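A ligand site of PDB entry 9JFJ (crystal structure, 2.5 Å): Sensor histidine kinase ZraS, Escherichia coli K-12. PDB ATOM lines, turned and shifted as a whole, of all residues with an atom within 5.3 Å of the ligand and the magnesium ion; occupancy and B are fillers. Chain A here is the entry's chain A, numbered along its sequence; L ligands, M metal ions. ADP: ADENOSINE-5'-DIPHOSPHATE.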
ATOM      1  N   ASN A 142     -15.706  18.602   5.312  1.00  0.00           N
ATOM      2  CA  ASN A 142     -16.910  19.143   5.974  1.00  0.00           C
ATOM      3  C   ASN A 142     -17.370  18.134   7.018  1.00  0.00           C
ATOM      4  O   ASN A 142     -17.590  18.503   8.173  1.00  0.00           O
ATOM      5  CB  ASN A 142     -18.016  19.459   4.970  1.00  0.00           C
ATOM      6  CG  ASN A 142     -18.309  20.930   4.801  1.00  0.00           C
ATOM      7  OD1 ASN A 142     -18.221  21.704   5.751  1.00  0.00           O
ATOM      8  ND2 ASN A 142     -18.668  21.322   3.591  1.00  0.00           N
ATOM      9  N   LEU A 143     -17.400  16.864   6.634  1.00  0.00           N
ATOM     10  CA  LEU A 143     -17.858  15.853   7.610  1.00  0.00           C
ATOM     11  C   LEU A 143     -16.889  15.829   8.790  1.00  0.00           C
ATOM     12  O   LEU A 143     -17.366  15.801   9.927  1.00  0.00           O
ATOM     13  CB  LEU A 143     -17.945  14.486   6.919  1.00  0.00           C
ATOM     14  CG  LEU A 143     -18.988  14.360   5.825  1.00  0.00           C
ATOM     15  CD1 LEU A 143     -18.939  12.970   5.201  1.00  0.00           C
ATOM     16  CD2 LEU A 143     -20.370  14.650   6.369  1.00  0.00           C
ATOM     17  N   ASN A 146     -17.351  18.760  11.089  1.00  0.00           N
ATOM     18  CA  ASN A 146     -18.593  18.624  11.869  1.00  0.00           C
ATOM     19  C   ASN A 146     -18.299  17.689  13.039  1.00  0.00           C
ATOM     20  O   ASN A 146     -18.621  18.029  14.204  1.00  0.00           O
ATOM     21  CB  ASN A 146     -19.695  18.091  10.966  1.00  0.00           C
ATOM     22  CG  ASN A 146     -20.415  19.156  10.187  1.00  0.00           C
ATOM     23  OD1 ASN A 146     -20.338  20.318  10.537  1.00  0.00           O
ATOM     24  ND2 ASN A 146     -21.132  18.764   9.153  1.00  0.00           N
ATOM     25  N   ALA A 147     -17.612  16.608  12.742  1.00  0.00           N
ATOM     26  CA  ALA A 147     -17.327  15.625  13.802  1.00  0.00           C
ATOM     27  C   ALA A 147     -16.464  16.285  14.873  1.00  0.00           C
ATOM     28  O   ALA A 147     -16.745  16.101  16.065  1.00  0.00           O
ATOM     29  CB  ALA A 147     -16.646  14.448  13.197  1.00  0.00           C
ATOM     30  N   GLN A 149     -16.161  19.415  15.672  1.00  0.00           N
ATOM     31  CA  GLN A 149     -16.860  20.435  16.475  1.00  0.00           C
ATOM     32  C   GLN A 149     -17.696  19.688  17.512  1.00  0.00           C
ATOM     33  O   GLN A 149     -17.549  20.021  18.712  1.00  0.00           O
ATOM     34  CB  GLN A 149     -17.648  21.329  15.509  1.00  0.00           C
ATOM     35  CG  GLN A 149     -16.777  22.261  14.696  1.00  0.00           C
ATOM     36  CD  GLN A 149     -17.503  22.755  13.475  1.00  0.00           C
ATOM     37  OE1 GLN A 149     -18.011  21.975  12.676  1.00  0.00           O
ATOM     38  NE2 GLN A 149     -17.544  24.066  13.306  1.00  0.00           N
ATOM     39  N   ALA A 150     -18.380  18.636  17.091  1.00  0.00           N
ATOM     40  CA  ALA A 150     -19.256  17.864  17.997  1.00  0.00           C
ATOM     41  C   ALA A 150     -18.517  17.194  19.150  1.00  0.00           C
ATOM     42  O   ALA A 150     -18.975  17.326  20.282  1.00  0.00           O
ATOM     43  CB  ALA A 150     -19.950  16.829  17.190  1.00  0.00           C
ATOM     44  N   ASP A 174     -18.072   9.377  14.260  1.00  0.00           N
ATOM     45  CA  ASP A 174     -17.547  10.232  15.338  1.00  0.00           C
ATOM     46  C   ASP A 174     -18.028   9.698  16.702  1.00  0.00           C
ATOM     47  O   ASP A 174     -18.782   8.736  16.703  1.00  0.00           O
ATOM     48  CB  ASP A 174     -17.979  11.684  15.142  1.00  0.00           C
ATOM     49  CG  ASP A 174     -19.464  11.946  15.151  1.00  0.00           C
ATOM     50  OD1 ASP A 174     -20.060  11.961  16.241  1.00  0.00           O
ATOM     51  OD2 ASP A 174     -20.012  12.193  14.062  1.00  0.00           O
ATOM     52  N   LYS A 177     -21.601  14.406  20.426  1.00  0.00           N
ATOM     53  CA  LYS A 177     -22.875  14.522  21.113  1.00  0.00           C
ATOM     54  C   LYS A 177     -24.017  13.816  20.404  1.00  0.00           C
ATOM     55  O   LYS A 177     -25.042  13.532  21.026  1.00  0.00           O
ATOM     56  CB  LYS A 177     -23.234  16.008  21.292  1.00  0.00           C
ATOM     57  CG  LYS A 177     -23.085  16.817  20.026  1.00  0.00           C
ATOM     58  CD  LYS A 177     -24.163  17.878  19.922  1.00  0.00           C
ATOM     59  CE  LYS A 177     -23.787  19.123  20.703  1.00  0.00           C
ATOM     60  NZ  LYS A 177     -24.598  20.298  20.280  1.00  0.00           N
ATOM     61  N   GLY A 178     -23.862  13.507  19.115  1.00  0.00           N
ATOM     62  CA  GLY A 178     -24.932  12.882  18.368  1.00  0.00           C
ATOM     63  C   GLY A 178     -26.032  13.869  18.013  1.00  0.00           C
ATOM     64  O   GLY A 178     -25.964  15.058  18.298  1.00  0.00           O
ATOM     65  N   ILE A 179     -27.070  13.335  17.372  1.00  0.00           N
ATOM     66  CA  ILE A 179     -28.231  14.135  16.972  1.00  0.00           C
ATOM     67  C   ILE A 179     -29.498  13.416  17.418  1.00  0.00           C
ATOM     68  O   ILE A 179     -29.597  12.190  17.324  1.00  0.00           O
ATOM     69  CB  ILE A 179     -28.284  14.410  15.447  1.00  0.00           C
ATOM     70  CG1 ILE A 179     -26.911  14.750  14.861  1.00  0.00           C
ATOM     71  CG2 ILE A 179     -29.267  15.516  15.152  1.00  0.00           C
ATOM     72  CD1 ILE A 179     -26.065  13.567  14.453  1.00  0.00           C
ATOM     73  N   GLN A 183     -34.311  16.031  15.194  1.00  0.00           N
ATOM     74  CA  GLN A 183     -33.444  16.820  14.331  1.00  0.00           C
ATOM     75  C   GLN A 183     -32.755  15.975  13.256  1.00  0.00           C
ATOM     76  O   GLN A 183     -32.039  16.525  12.417  1.00  0.00           O
ATOM     77  CB  GLN A 183     -32.390  17.547  15.169  1.00  0.00           C
ATOM     78  CG  GLN A 183     -32.929  18.693  15.994  1.00  0.00           C
ATOM     79  CD  GLN A 183     -31.856  19.359  16.820  1.00  0.00           C
ATOM     80  OE1 GLN A 183     -30.851  18.741  17.178  1.00  0.00           O
ATOM     81  NE2 GLN A 183     -32.066  20.637  17.144  1.00  0.00           N
ATOM     82  N   ILE A 187     -31.205  17.978   9.612  1.00  0.00           N
ATOM     83  CA  ILE A 187     -29.760  18.061   9.648  1.00  0.00           C
ATOM     84  C   ILE A 187     -29.171  18.403   8.289  1.00  0.00           C
ATOM     85  O   ILE A 187     -28.196  19.166   8.217  1.00  0.00           O
ATOM     86  CB  ILE A 187     -29.206  16.735  10.209  1.00  0.00           C
ATOM     87  CG1 ILE A 187     -27.689  16.747  10.272  1.00  0.00           C
ATOM     88  CG2 ILE A 187     -29.728  15.551   9.423  1.00  0.00           C
ATOM     89  CD1 ILE A 187     -27.098  15.397  10.602  1.00  0.00           C
ATOM     90  N   THR A 189     -30.965  20.040   6.049  1.00  0.00           N
ATOM     91  CA  THR A 189     -31.726  21.162   5.548  1.00  0.00           C
ATOM     92  C   THR A 189     -30.842  22.411   5.486  1.00  0.00           C
ATOM     93  O   THR A 189     -30.086  22.685   6.417  1.00  0.00           O
ATOM     94  CB  THR A 189     -32.943  21.427   6.424  1.00  0.00           C
ATOM     95  OG1 THR A 189     -33.862  20.331   6.305  1.00  0.00           O
ATOM     96  CG2 THR A 189     -33.652  22.703   6.011  1.00  0.00           C
ATOM     97  N   PHE A 192     -29.772  25.400   8.525  1.00  0.00           N
ATOM     98  CA  PHE A 192     -30.081  24.867   9.844  1.00  0.00           C
ATOM     99  C   PHE A 192     -28.784  24.566  10.578  1.00  0.00           C
ATOM    100  O   PHE A 192     -27.966  23.773  10.103  1.00  0.00           O
ATOM    101  CB  PHE A 192     -30.925  23.597   9.750  1.00  0.00           C
ATOM    102  CG  PHE A 192     -31.121  22.906  11.061  1.00  0.00           C
ATOM    103  CD1 PHE A 192     -31.953  23.459  12.026  1.00  0.00           C
ATOM    104  CD2 PHE A 192     -30.459  21.725  11.356  1.00  0.00           C
ATOM    105  CE1 PHE A 192     -32.126  22.833  13.236  1.00  0.00           C
ATOM    106  CE2 PHE A 192     -30.632  21.098  12.567  1.00  0.00           C
ATOM    107  CZ  PHE A 192     -31.471  21.653  13.511  1.00  0.00           C
ATOM    108  N   THR A 193     -28.598  25.189  11.737  1.00  0.00           N
ATOM    109  CA  THR A 193     -27.414  24.936  12.535  1.00  0.00           C
ATOM    110  C   THR A 193     -27.749  25.086  14.006  1.00  0.00           C
ATOM    111  O   THR A 193     -28.656  25.841  14.393  1.00  0.00           O
ATOM    112  CB  THR A 193     -26.260  25.875  12.146  1.00  0.00           C
ATOM    113  OG1 THR A 193     -25.040  25.407  12.738  1.00  0.00           O
ATOM    114  CG2 THR A 193     -26.538  27.300  12.576  1.00  0.00           C
ATOM    115  N   THR A 194     -27.022  24.313  14.819  1.00  0.00           N
ATOM    116  CA  THR A 194     -27.142  24.395  16.283  1.00  0.00           C
ATOM    117  C   THR A 194     -25.934  25.185  16.814  1.00  0.00           C
ATOM    118  O   THR A 194     -25.731  25.139  18.031  1.00  0.00           O
ATOM    119  CB  THR A 194     -26.954  23.001  16.877  1.00  0.00           C
ATOM    120  OG1 THR A 194     -25.792  22.409  16.313  1.00  0.00           O
ATOM    121  CG2 THR A 194     -28.147  22.100  16.637  1.00  0.00           C
ATOM    122  N   LYS A 195     -25.175  25.867  15.946  1.00  0.00           N
ATOM    123  CA  LYS A 195     -23.947  26.566  16.368  1.00  0.00           C
ATOM    124  C   LYS A 195     -24.071  28.059  16.088  1.00  0.00           C
ATOM    125  O   LYS A 195     -24.614  28.412  15.045  1.00  0.00           O
ATOM    126  CB  LYS A 195     -22.775  25.938  15.622  1.00  0.00           C
ATOM    127  CG  LYS A 195     -22.842  24.425  15.449  1.00  0.00           C
ATOM    128  CD  LYS A 195     -21.735  23.919  14.580  1.00  0.00           C
ATOM    129  CE  LYS A 195     -21.677  22.420  14.537  1.00  0.00           C
ATOM    130  NZ  LYS A 195     -20.685  21.955  13.552  1.00  0.00           N
ATOM    131  N   GLY A 198     -22.066  28.934  13.083  1.00  0.00           N
ATOM    132  CA  GLY A 198     -22.236  27.882  12.076  1.00  0.00           C
ATOM    133  C   GLY A 198     -22.957  28.359  10.842  1.00  0.00           C
ATOM    134  O   GLY A 198     -23.736  29.299  10.924  1.00  0.00           O
ATOM    135  N   THR A 199     -22.632  27.732   9.724  1.00  0.00           N
ATOM    136  CA  THR A 199     -23.339  28.021   8.463  1.00  0.00           C
ATOM    137  C   THR A 199     -24.153  26.766   8.277  1.00  0.00           C
ATOM    138  O   THR A 199     -23.576  25.698   8.389  1.00  0.00           O
ATOM    139  CB  THR A 199     -22.336  28.062   7.312  1.00  0.00           C
ATOM    140  OG1 THR A 199     -21.769  26.781   7.110  1.00  0.00           O
ATOM    141  CG2 THR A 199     -21.226  29.070   7.551  1.00  0.00           C
ATOM    142  N   GLY A 200     -25.456  26.870   8.119  1.00  0.00           N
ATOM    143  CA  GLY A 200     -26.168  25.591   8.002  1.00  0.00           C
ATOM    144  C   GLY A 200     -26.166  25.121   6.577  1.00  0.00           C
ATOM    145  O   GLY A 200     -27.225  24.754   6.090  1.00  0.00           O
ATOM    146  N   LEU A 201     -25.006  25.063   5.964  1.00  0.00           N
ATOM    147  CA  LEU A 201     -24.985  24.770   4.517  1.00  0.00           C
ATOM    148  C   LEU A 201     -23.838  23.823   4.239  1.00  0.00           C
ATOM    149  O   LEU A 201     -23.620  23.505   3.084  1.00  0.00           O
ATOM    150  CB  LEU A 201     -24.813  26.097   3.774  1.00  0.00           C
ATOM    151  CG  LEU A 201     -25.952  27.100   3.862  1.00  0.00           C
ATOM    152  CD1 LEU A 201     -25.529  28.436   3.308  1.00  0.00           C
ATOM    153  CD2 LEU A 201     -27.180  26.587   3.118  1.00  0.00           C
ATOM    154  N   GLY A 202     -23.149  23.387   5.279  1.00  0.00           N
ATOM    155  CA  GLY A 202     -22.088  22.430   5.032  1.00  0.00           C
ATOM    156  C   GLY A 202     -22.605  21.090   4.569  1.00  0.00           C
ATOM    157  O   GLY A 202     -22.107  20.505   3.602  1.00  0.00           O
ATOM    158  N   LEU A 203     -23.628  20.566   5.253  1.00  0.00           N
ATOM    159  CA  LEU A 203     -24.210  19.310   4.818  1.00  0.00           C
ATOM    160  C   LEU A 203     -25.069  19.490   3.576  1.00  0.00           C
ATOM    161  O   LEU A 203     -25.237  18.530   2.804  1.00  0.00           O
ATOM    162  CB  LEU A 203     -25.033  18.697   5.953  1.00  0.00           C
ATOM    163  CG  LEU A 203     -24.201  17.809   6.882  1.00  0.00           C
ATOM    164  CD1 LEU A 203     -25.056  17.312   8.023  1.00  0.00           C
ATOM    165  CD2 LEU A 203     -23.613  16.637   6.128  1.00  0.00           C
ATOM    166  N   ALA A 204     -25.579  20.704   3.335  1.00  0.00           N
ATOM    167  CA  ALA A 204     -26.217  20.989   2.047  1.00  0.00           C
ATOM    168  C   ALA A 204     -25.204  20.851   0.908  1.00  0.00           C
ATOM    169  O   ALA A 204     -25.507  20.254  -0.126  1.00  0.00           O
ATOM    170  CB  ALA A 204     -26.829  22.386   2.072  1.00  0.00           C
ATOM    171  N   SER A 227     -22.237   9.386  16.096  1.00  0.00           N
ATOM    172  CA  SER A 227     -22.894   9.427  14.796  1.00  0.00           C
ATOM    173  C   SER A 227     -22.006   8.781  13.733  1.00  0.00           C
ATOM    174  O   SER A 227     -20.794   8.665  13.913  1.00  0.00           O
ATOM    175  CB  SER A 227     -23.231  10.858  14.374  1.00  0.00           C
ATOM    176  OG  SER A 227     -23.791  11.582  15.444  1.00  0.00           O
ATOM    177  N   PHE A 229     -21.739   8.843   9.374  1.00  0.00           N
ATOM    178  CA  PHE A 229     -22.204   9.346   8.061  1.00  0.00           C
ATOM    179  C   PHE A 229     -21.650   8.392   7.005  1.00  0.00           C
ATOM    180  O   PHE A 229     -20.440   8.207   6.958  1.00  0.00           O
ATOM    181  CB  PHE A 229     -21.764  10.791   7.843  1.00  0.00           C
ATOM    182  CG  PHE A 229     -22.558  11.833   8.597  1.00  0.00           C
ATOM    183  CD1 PHE A 229     -22.339  12.070   9.935  1.00  0.00           C
ATOM    184  CD2 PHE A 229     -23.514  12.586   7.945  1.00  0.00           C
ATOM    185  CE1 PHE A 229     -23.053  13.026  10.624  1.00  0.00           C
ATOM    186  CE2 PHE A 229     -24.228  13.555   8.630  1.00  0.00           C
ATOM    187  CZ  PHE A 229     -23.998  13.778   9.963  1.00  0.00           C
HETATM  188  PB  ADP L   1     -22.835  23.569  10.651  1.00  0.00           P
HETATM  189  O1B ADP L   1     -21.724  22.614  10.741  1.00  0.00           O
HETATM  190  O2B ADP L   1     -23.803  23.425  11.763  1.00  0.00           O
HETATM  191  O3B ADP L   1     -22.356  24.963  10.518  1.00  0.00           O
HETATM  192  PA  ADP L   1     -23.997  21.690   8.744  1.00  0.00           P
HETATM  193  O1A ADP L   1     -25.088  21.847   7.743  1.00  0.00           O
HETATM  194  O2A ADP L   1     -22.725  21.063   8.297  1.00  0.00           O
HETATM  195  O3A ADP L   1     -23.666  23.126   9.355  1.00  0.00           O
HETATM  196  O5' ADP L   1     -24.557  20.916  10.025  1.00  0.00           O
HETATM  197  C5' ADP L   1     -25.956  21.035  10.342  1.00  0.00           C
HETATM  198  C4' ADP L   1     -26.227  20.450  11.710  1.00  0.00           C
HETATM  199  O4' ADP L   1     -26.078  19.014  11.645  1.00  0.00           O
HETATM  200  C3' ADP L   1     -25.265  20.860  12.820  1.00  0.00           C
HETATM  201  O3' ADP L   1     -25.632  22.109  13.379  1.00  0.00           O
HETATM  202  C2' ADP L   1     -25.429  19.712  13.823  1.00  0.00           C
HETATM  203  O2' ADP L   1     -26.542  19.909  14.674  1.00  0.00           O
HETATM  204  C1' ADP L   1     -25.691  18.520  12.912  1.00  0.00           C
HETATM  205  N9  ADP L   1     -24.542  17.651  12.716  1.00  0.00           N
HETATM  206  C8  ADP L   1     -23.865  17.452  11.545  1.00  0.00           C
HETATM  207  N7  ADP L   1     -22.877  16.597  11.642  1.00  0.00           N
HETATM  208  C5  ADP L   1     -22.906  16.208  12.975  1.00  0.00           C
HETATM  209  C6  ADP L   1     -22.104  15.309  13.710  1.00  0.00           C
HETATM  210  N6  ADP L   1     -21.101  14.634  13.187  1.00  0.00           N
HETATM  211  N1  ADP L   1     -22.410  15.136  15.010  1.00  0.00           N
HETATM  212  C2  ADP L   1     -23.426  15.826  15.538  1.00  0.00           C
HETATM  213  N3  ADP L   1     -24.243  16.692  14.941  1.00  0.00           N
HETATM  214  C4  ADP L   1     -23.931  16.843  13.642  1.00  0.00           C
HETATM  215 MG    MG M   1     -20.849  21.812   9.027  1.00  0.00          MG
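An oxygen (O3') of the ligand lies within hydrogen-bond range of the backbone NH (N) of Thr 194, 3.0 Å away.
The side-chain hydroxyl of Thr 193 sits at hydrogen-bond distance from an oxygen (O2B) of the ligand (2.5 Å).
An oxygen (O2B) of the ligand lies within salt-bridge range of the side-chain amino group (NZ) of Lys 195, at 3.9 Å.
An oxygen (O3B) of the ligand sits close to the backbone carbonyl oxygen of Thr 199, at 2.6 Å.
An oxygen (O3B) of the ligand lies within hydrogen-bond range of the backbone NH (N) of Thr 199.
The backbone NH of Gly 202 sits at hydrogen-bond distance from an oxygen (O1A) of the ligand, 3.5 Å away.
An oxygen (O1A) of the ligand sits at hydrogen-bond distance from the backbone NH (N) of Leu 203, at 3.2 Å.
The side-chain carboxylate of Asp 174 sits at hydrogen-bond distance from a nitrogen (N6) of the ligand, at 2.8 Å.
O3' of the ligand is in hydrogen-bond range of OG1 of Thr 194 (3.0 Å).
The side-chain amide oxygen (OD1) of Asn 146 sits close to the side-chain amino group (NZ) of Lys 195, 3.4 Å away.
The side-chain hydroxyl (OG1) of Thr 193 is in hydrogen-bond range of the backbone NH (N) of Lys 195.
O of Ser 227 lies within hydrogen-bond range of N of Asp 174 (2.8 Å).
The side-chain amino group of Lys 195 sits at hydrogen-bond distance from the side-chain amide oxygen of Gln 149, at 2.8 Å.
Merely in contact with the ligand: Ala 147, Ala 150, Gly 178, Ile 179, Ile 187, Phe 192, Gly 198, Gly 200, Leu 201, Ser 227 and Phe 229.
Hydrophobic or aromatic side chains within 4 Å of the ligand: Ala 150, Ile 179, Ile 187, Leu 203 and Phe 229.
Within 4 Å of the ligand: Asn 146, Ala 147, Ala 150, Asp 174, Gly 178, Ile 179, Ile 187, Phe 192, Thr 193, Thr 194, Lys 195, Gly 198, Thr 199, Gly 200, Leu 201, Gly 202, Leu 203, Ser 227 and Phe 229.
The nearest printed residue that does not touch the ligand is Gln 149 (4.2 Å).
One residue has an atom within 4 Å of the magnesium ion: Asn 146.
The magnesium ion is bound by O1B of the ligand (2.1 Å), O2A of the ligand (2.1 Å) and OD1 of Asn 146 (2.2 Å).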
